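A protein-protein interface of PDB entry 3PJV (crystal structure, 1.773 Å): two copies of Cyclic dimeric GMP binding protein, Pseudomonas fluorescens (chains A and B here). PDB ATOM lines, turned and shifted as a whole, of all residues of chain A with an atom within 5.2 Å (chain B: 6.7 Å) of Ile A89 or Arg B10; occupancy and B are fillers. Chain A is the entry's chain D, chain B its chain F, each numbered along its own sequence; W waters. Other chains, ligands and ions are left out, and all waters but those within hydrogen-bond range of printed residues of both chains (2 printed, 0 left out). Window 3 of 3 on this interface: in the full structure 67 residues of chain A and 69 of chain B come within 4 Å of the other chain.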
ATOM      1  N   PHE A  85     -31.205   0.352  14.437  1.00  0.00           N
ATOM      2  CA  PHE A  85     -30.570   1.633  14.745  1.00  0.00           C
ATOM      3  C   PHE A  85     -29.063   1.575  14.482  1.00  0.00           C
ATOM      4  O   PHE A  85     -28.456   2.556  14.049  1.00  0.00           O
ATOM      5  CB  PHE A  85     -30.857   2.054  16.191  1.00  0.00           C
ATOM      6  CG  PHE A  85     -30.257   3.393  16.572  1.00  0.00           C
ATOM      7  CD1 PHE A  85     -30.826   4.572  16.108  1.00  0.00           C
ATOM      8  CD2 PHE A  85     -29.149   3.471  17.396  1.00  0.00           C
ATOM      9  CE1 PHE A  85     -30.289   5.801  16.446  1.00  0.00           C
ATOM     10  CE2 PHE A  85     -28.608   4.704  17.757  1.00  0.00           C
ATOM     11  CZ  PHE A  85     -29.184   5.871  17.273  1.00  0.00           C
ATOM     12  N   VAL A  86     -28.465   0.412  14.726  1.00  0.00           N
ATOM     13  CA  VAL A  86     -27.054   0.205  14.429  1.00  0.00           C
ATOM     14  C   VAL A  86     -26.738   0.451  12.960  1.00  0.00           C
ATOM     15  O   VAL A  86     -25.788   1.162  12.633  1.00  0.00           O
ATOM     16  CB  VAL A  86     -26.592  -1.217  14.812  1.00  0.00           C
ATOM     17  CG1 VAL A  86     -25.096  -1.371  14.588  1.00  0.00           C
ATOM     18  CG2 VAL A  86     -26.931  -1.498  16.252  1.00  0.00           C
ATOM     19  N   LYS A  87     -27.539  -0.143  12.076  1.00  0.00           N
ATOM     20  CA  LYS A  87     -27.369   0.046  10.641  1.00  0.00           C
ATOM     21  C   LYS A  87     -27.568   1.511  10.281  1.00  0.00           C
ATOM     22  O   LYS A  87     -26.796   2.084   9.509  1.00  0.00           O
ATOM     23  CB  LYS A  87     -28.373  -0.814   9.867  1.00  0.00           C
ATOM     24  CG  LYS A  87     -28.548  -2.215  10.433  1.00  0.00           C
ATOM     25  CD  LYS A  87     -29.630  -2.983   9.678  1.00  0.00           C
ATOM     26  CE  LYS A  87     -30.942  -2.217   9.683  1.00  0.00           C
ATOM     27  NZ  LYS A  87     -32.032  -2.942   8.980  1.00  0.00           N
ATOM     28  N   LEU A  88     -28.609   2.112  10.851  1.00  0.00           N
ATOM     29  CA  LEU A  88     -28.923   3.515  10.608  1.00  0.00           C
ATOM     30  C   LEU A  88     -27.757   4.425  10.987  1.00  0.00           C
ATOM     31  O   LEU A  88     -27.322   5.250  10.185  1.00  0.00           O
ATOM     32  CB  LEU A  88     -30.188   3.915  11.376  1.00  0.00           C
ATOM     33  CG  LEU A  88     -30.780   5.308  11.163  1.00  0.00           C
ATOM     34  CD1 LEU A  88     -31.143   5.535   9.701  1.00  0.00           C
ATOM     35  CD2 LEU A  88     -32.006   5.499  12.054  1.00  0.00           C
ATOM     36  N   ILE A  89     -27.252   4.268  12.211  1.00  0.00           N
ATOM     37  CA  ILE A  89     -26.117   5.060  12.672  1.00  0.00           C
ATOM     38  C   ILE A  89     -24.852   4.712  11.882  1.00  0.00           C
ATOM     39  O   ILE A  89     -24.094   5.594  11.503  1.00  0.00           O
ATOM     40  CB  ILE A  89     -25.889   4.891  14.197  1.00  0.00           C
ATOM     41  CG1 ILE A  89     -26.147   6.212  14.917  1.00  0.00           C
ATOM     42  CG2 ILE A  89     -24.478   4.437  14.492  1.00  0.00           C
ATOM     43  CD1 ILE A  89     -27.463   6.827  14.605  1.00  0.00           C
ATOM     44  N   GLY A  90     -24.638   3.426  11.624  1.00  0.00           N
ATOM     45  CA  GLY A  90     -23.491   2.979  10.854  1.00  0.00           C
ATOM     46  C   GLY A  90     -22.170   3.467  11.424  1.00  0.00           C
ATOM     47  O   GLY A  90     -21.426   4.189  10.761  1.00  0.00           O
ATOM     48  N   LEU A  91     -21.890   3.083  12.665  1.00  0.00           N
ATOM     49  CA  LEU A  91     -20.625   3.411  13.315  1.00  0.00           C
ATOM     50  C   LEU A  91     -19.456   2.654  12.697  1.00  0.00           C
ATOM     51  O   LEU A  91     -19.526   1.442  12.496  1.00  0.00           O
ATOM     52  CB  LEU A  91     -20.695   3.061  14.801  1.00  0.00           C
ATOM     53  CG  LEU A  91     -20.849   4.183  15.822  1.00  0.00           C
ATOM     54  CD1 LEU A  91     -20.392   3.678  17.178  1.00  0.00           C
ATOM     55  CD2 LEU A  91     -20.040   5.386  15.413  1.00  0.00           C
ATOM     56  N   GLU A  92     -18.371   3.366  12.409  1.00  0.00           N
ATOM     57  CA  GLU A  92     -17.150   2.715  11.942  1.00  0.00           C
ATOM     58  C   GLU A  92     -16.448   2.039  13.113  1.00  0.00           C
ATOM     59  O   GLU A  92     -16.479   2.546  14.230  1.00  0.00           O
ATOM     60  CB  GLU A  92     -16.207   3.726  11.295  1.00  0.00           C
ATOM     61  CG  GLU A  92     -15.456   4.584  12.293  1.00  0.00           C
ATOM     62  CD  GLU A  92     -14.440   5.486  11.626  1.00  0.00           C
ATOM     63  OE1 GLU A  92     -13.226   5.217  11.751  1.00  0.00           O
ATOM     64  OE2 GLU A  92     -14.857   6.464  10.976  1.00  0.00           O
ATOM     65  N   LEU A 120     -23.135   2.993  21.319  1.00  0.00           N
ATOM     66  CA  LEU A 120     -24.458   2.858  20.701  1.00  0.00           C
ATOM     67  C   LEU A 120     -25.572   3.193  21.685  1.00  0.00           C
ATOM     68  O   LEU A 120     -26.566   3.832  21.315  1.00  0.00           O
ATOM     69  CB  LEU A 120     -24.641   1.456  20.130  1.00  0.00           C
ATOM     70  CG  LEU A 120     -23.804   1.194  18.878  1.00  0.00           C
ATOM     71  CD1 LEU A 120     -23.679  -0.294  18.608  1.00  0.00           C
ATOM     72  CD2 LEU A 120     -24.416   1.941  17.689  1.00  0.00           C
ATOM     73  N   LEU A 123     -25.805   6.947  21.944  1.00  0.00           N
ATOM     74  CA  LEU A 123     -26.356   7.527  20.726  1.00  0.00           C
ATOM     75  C   LEU A 123     -27.868   7.336  20.681  1.00  0.00           C
ATOM     76  O   LEU A 123     -28.606   8.247  20.306  1.00  0.00           O
ATOM     77  CB  LEU A 123     -25.704   6.903  19.487  1.00  0.00           C
ATOM     78  CG  LEU A 123     -24.297   7.414  19.185  1.00  0.00           C
ATOM     79  CD1 LEU A 123     -23.621   6.514  18.174  1.00  0.00           C
ATOM     80  CD2 LEU A 123     -24.351   8.855  18.697  1.00  0.00           C
ATOM     81  N   MET B   3     -30.649  13.455  11.002  1.00  0.00           N
ATOM     82  CA  MET B   3     -29.654  12.642  11.692  1.00  0.00           C
ATOM     83  C   MET B   3     -28.242  13.158  11.440  1.00  0.00           C
ATOM     84  O   MET B   3     -27.298  12.377  11.316  1.00  0.00           O
ATOM     85  CB  MET B   3     -29.768  11.181  11.260  1.00  0.00           C
ATOM     86  CG  MET B   3     -31.120  10.545  11.560  1.00  0.00           C
ATOM     87  SD  MET B   3     -31.207   9.601  13.275  1.00  0.00           S
ATOM     88  CE  MET B   3     -30.968  11.102  14.511  1.00  0.00           C
ATOM     89  N   LEU B   6     -26.403  14.384  15.290  1.00  0.00           N
ATOM     90  CA  LEU B   6     -25.586  13.485  16.096  1.00  0.00           C
ATOM     91  C   LEU B   6     -24.181  13.309  15.519  1.00  0.00           C
ATOM     92  O   LEU B   6     -23.378  12.538  16.040  1.00  0.00           O
ATOM     93  CB  LEU B   6     -26.277  12.129  16.251  1.00  0.00           C
ATOM     94  CG  LEU B   6     -27.578  12.124  17.058  1.00  0.00           C
ATOM     95  CD1 LEU B   6     -28.263  10.766  16.981  1.00  0.00           C
ATOM     96  CD2 LEU B   6     -27.323  12.516  18.506  1.00  0.00           C
ATOM     97  N   GLU B   7     -23.888  14.036  14.446  1.00  0.00           N
ATOM     98  CA  GLU B   7     -22.583  13.974  13.798  1.00  0.00           C
ATOM     99  C   GLU B   7     -21.423  14.213  14.771  1.00  0.00           C
ATOM    100  O   GLU B   7     -20.432  13.482  14.762  1.00  0.00           O
ATOM    101  CB  GLU B   7     -22.516  14.989  12.656  1.00  0.00           C
ATOM    102  CG  GLU B   7     -22.353  14.381  11.277  1.00  0.00           C
ATOM    103  CD  GLU B   7     -20.945  13.879  11.017  1.00  0.00           C
ATOM    104  OE1 GLU B   7     -20.339  13.280  11.932  1.00  0.00           O
ATOM    105  OE2 GLU B   7     -20.441  14.089   9.891  1.00  0.00           O
ATOM    106  N   SER B   8     -21.538  15.244  15.601  1.00  0.00           N
ATOM    107  CA  SER B   8     -20.454  15.576  16.522  1.00  0.00           C
ATOM    108  C   SER B   8     -20.323  14.525  17.624  1.00  0.00           C
ATOM    109  O   SER B   8     -19.212  14.162  18.008  1.00  0.00           O
ATOM    110  CB  SER B   8     -20.635  16.978  17.109  1.00  0.00           C
ATOM    111  OG  SER B   8     -21.865  17.090  17.799  1.00  0.00           O
ATOM    112  N   SER B   9     -21.457  14.042  18.126  1.00  0.00           N
ATOM    113  CA  SER B   9     -21.466  12.935  19.079  1.00  0.00           C
ATOM    114  C   SER B   9     -20.809  11.699  18.492  1.00  0.00           C
ATOM    115  O   SER B   9     -20.079  10.991  19.181  1.00  0.00           O
ATOM    116  CB  SER B   9     -22.895  12.580  19.493  1.00  0.00           C
ATOM    117  OG  SER B   9     -23.341  13.398  20.555  1.00  0.00           O
ATOM    118  N   ARG B  10     -21.080  11.434  17.216  1.00  0.00           N
ATOM    119  CA  ARG B  10     -20.530  10.261  16.547  1.00  0.00           C
ATOM    120  C   ARG B  10     -19.009  10.308  16.437  1.00  0.00           C
ATOM    121  O   ARG B  10     -18.326   9.331  16.744  1.00  0.00           O
ATOM    122  CB  ARG B  10     -21.128  10.100  15.151  1.00  0.00           C
ATOM    123  CG  ARG B  10     -20.359   9.098  14.299  1.00  0.00           C
ATOM    124  CD  ARG B  10     -20.534   9.367  12.814  1.00  0.00           C
ATOM    125  NE  ARG B  10     -21.930   9.256  12.412  1.00  0.00           N
ATOM    126  CZ  ARG B  10     -22.503   8.126  12.012  1.00  0.00           C
ATOM    127  NH1 ARG B  10     -21.795   6.997  11.958  1.00  0.00           N
ATOM    128  NH2 ARG B  10     -23.784   8.124  11.665  1.00  0.00           N
ATOM    129  N   THR B  11     -18.466  11.432  15.984  1.00  0.00           N
ATOM    130  CA  THR B  11     -17.023  11.498  15.821  1.00  0.00           C
ATOM    131  C   THR B  11     -16.324  11.395  17.177  1.00  0.00           C
ATOM    132  O   THR B  11     -15.270  10.778  17.288  1.00  0.00           O
ATOM    133  CB  THR B  11     -16.569  12.744  15.039  1.00  0.00           C
ATOM    134  OG1 THR B  11     -17.638  13.690  14.985  1.00  0.00           O
ATOM    135  CG2 THR B  11     -16.197  12.359  13.611  1.00  0.00           C
ATOM    136  N   GLN B  12     -16.928  11.980  18.205  1.00  0.00           N
ATOM    137  CA  GLN B  12     -16.381  11.882  19.552  1.00  0.00           C
ATOM    138  C   GLN B  12     -16.321  10.440  20.058  1.00  0.00           C
ATOM    139  O   GLN B  12     -15.314  10.016  20.630  1.00  0.00           O
ATOM    140  CB  GLN B  12     -17.177  12.741  20.533  1.00  0.00           C
ATOM    141  CG  GLN B  12     -17.166  12.175  21.945  1.00  0.00           C
ATOM    142  CD  GLN B  12     -17.727  13.131  22.977  1.00  0.00           C
ATOM    143  OE1 GLN B  12     -18.048  14.281  22.670  1.00  0.00           O
ATOM    144  NE2 GLN B  12     -17.846  12.658  24.212  1.00  0.00           N
ATOM    145  N   TYR B  13     -17.399   9.686  19.864  1.00  0.00           N
ATOM    146  CA  TYR B  13     -17.424   8.299  20.324  1.00  0.00           C
ATOM    147  C   TYR B  13     -16.455   7.446  19.509  1.00  0.00           C
ATOM    148  O   TYR B  13     -15.774   6.571  20.039  1.00  0.00           O
ATOM    149  CB  TYR B  13     -18.839   7.717  20.250  1.00  0.00           C
ATOM    150  CG  TYR B  13     -19.871   8.487  21.032  1.00  0.00           C
ATOM    151  CD1 TYR B  13     -19.504   9.447  21.967  1.00  0.00           C
ATOM    152  CD2 TYR B  13     -21.222   8.260  20.829  1.00  0.00           C
ATOM    153  CE1 TYR B  13     -20.458  10.157  22.674  1.00  0.00           C
ATOM    154  CE2 TYR B  13     -22.180   8.960  21.530  1.00  0.00           C
ATOM    155  CZ  TYR B  13     -21.796   9.906  22.449  1.00  0.00           C
ATOM    156  OH  TYR B  13     -22.762  10.601  23.139  1.00  0.00           O
ATOM    157  N   VAL B  14     -16.388   7.706  18.210  1.00  0.00           N
ATOM    158  CA  VAL B  14     -15.424   7.016  17.367  1.00  0.00           C
ATOM    159  C   VAL B  14     -13.993   7.298  17.823  1.00  0.00           C
ATOM    160  O   VAL B  14     -13.152   6.395  17.847  1.00  0.00           O
ATOM    161  CB  VAL B  14     -15.585   7.422  15.887  1.00  0.00           C
ATOM    162  CG1 VAL B  14     -14.361   7.019  15.090  1.00  0.00           C
ATOM    163  CG2 VAL B  14     -16.829   6.789  15.319  1.00  0.00           C
ATOM    164  N   ASN B  15     -13.711   8.548  18.184  1.00  0.00           N
ATOM    165  CA  ASN B  15     -12.381   8.890  18.683  1.00  0.00           C
ATOM    166  C   ASN B  15     -12.058   8.113  19.943  1.00  0.00           C
ATOM    167  O   ASN B  15     -10.932   7.652  20.124  1.00  0.00           O
ATOM    168  CB  ASN B  15     -12.241  10.393  18.951  1.00  0.00           C
ATOM    169  CG  ASN B  15     -12.097  11.205  17.672  1.00  0.00           C
ATOM    170  OD1 ASN B  15     -11.915  10.649  16.588  1.00  0.00           O
ATOM    171  ND2 ASN B  15     -12.170  12.523  17.795  1.00  0.00           N
HETATM  172  O   HOH W   1     -19.041   6.546  12.106  1.00  0.00           O
HETATM  173  O   HOH W   2     -26.033   7.491   9.517  1.00  0.00           O
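NH1 of Arg B10 lies within hydrogen-bond range of O of Gly A90, 3.1 Å away. The backbone carbonyl oxygen of Ile A89 sits at hydrogen-bond distance from the guanidinium group of Arg B10 (2.6 Å).
Of chain B, only Arg B10 (2.6 Å) comes within 4 Å of Ile A89. Of chain A, only Ile A89, Gly A90 and Leu A91 come within 4 Å of Arg B10. Of the printed residues of chain B, Gly A90 touches Arg B10 (3.1 Å). Of the printed residues of chain B, Leu A91 touches Arg B10 (3.9 Å) and Val B14 (3.5 Å). Printed residues of chain A within 4 Å of Tyr B13: Leu A123. Met B3 touches none of the printed residues of chain A. The nearest residue of chain A that does not touch Arg B10 is Leu A123 (4.4 Å). The nearest printed residue of chain B that does not touch Glu A92 is Arg B10 (5.0 Å).
CG of Arg B10 touches CD2 of Leu A91, at 3.9 Å. Leu A91 touches Val B14 (CD2 to CG2, 3.5 Å). CD of Glu A92 touches CG1 of Val B14 (3.8 Å). Leu A123 touches Tyr B13.
Water W2 lies within hydrogen-bond range of the backbone carbonyl oxygen (O) of Leu A88 (2.7 Å), the guanidinium group (NH2) of Arg B10 (3.2 Å) and the backbone carbonyl oxygen (O) of Ile A89 (3.4 Å). Water W1 lies within hydrogen-bond range of NH1 of Arg B10 and N of Glu A92.
Of the 11 printed residues of chain B, 3 touch a printed residue of chain A. Among the printed residues, no Asp or Glu carboxylate lies within 4 Å of a Lys or Arg side-chain nitrogen of the other chain.
No position is printed for both chains. Of the 6 pairs that touch across the chains among the printed residues, none has its exchanged pair printed and touching as well.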
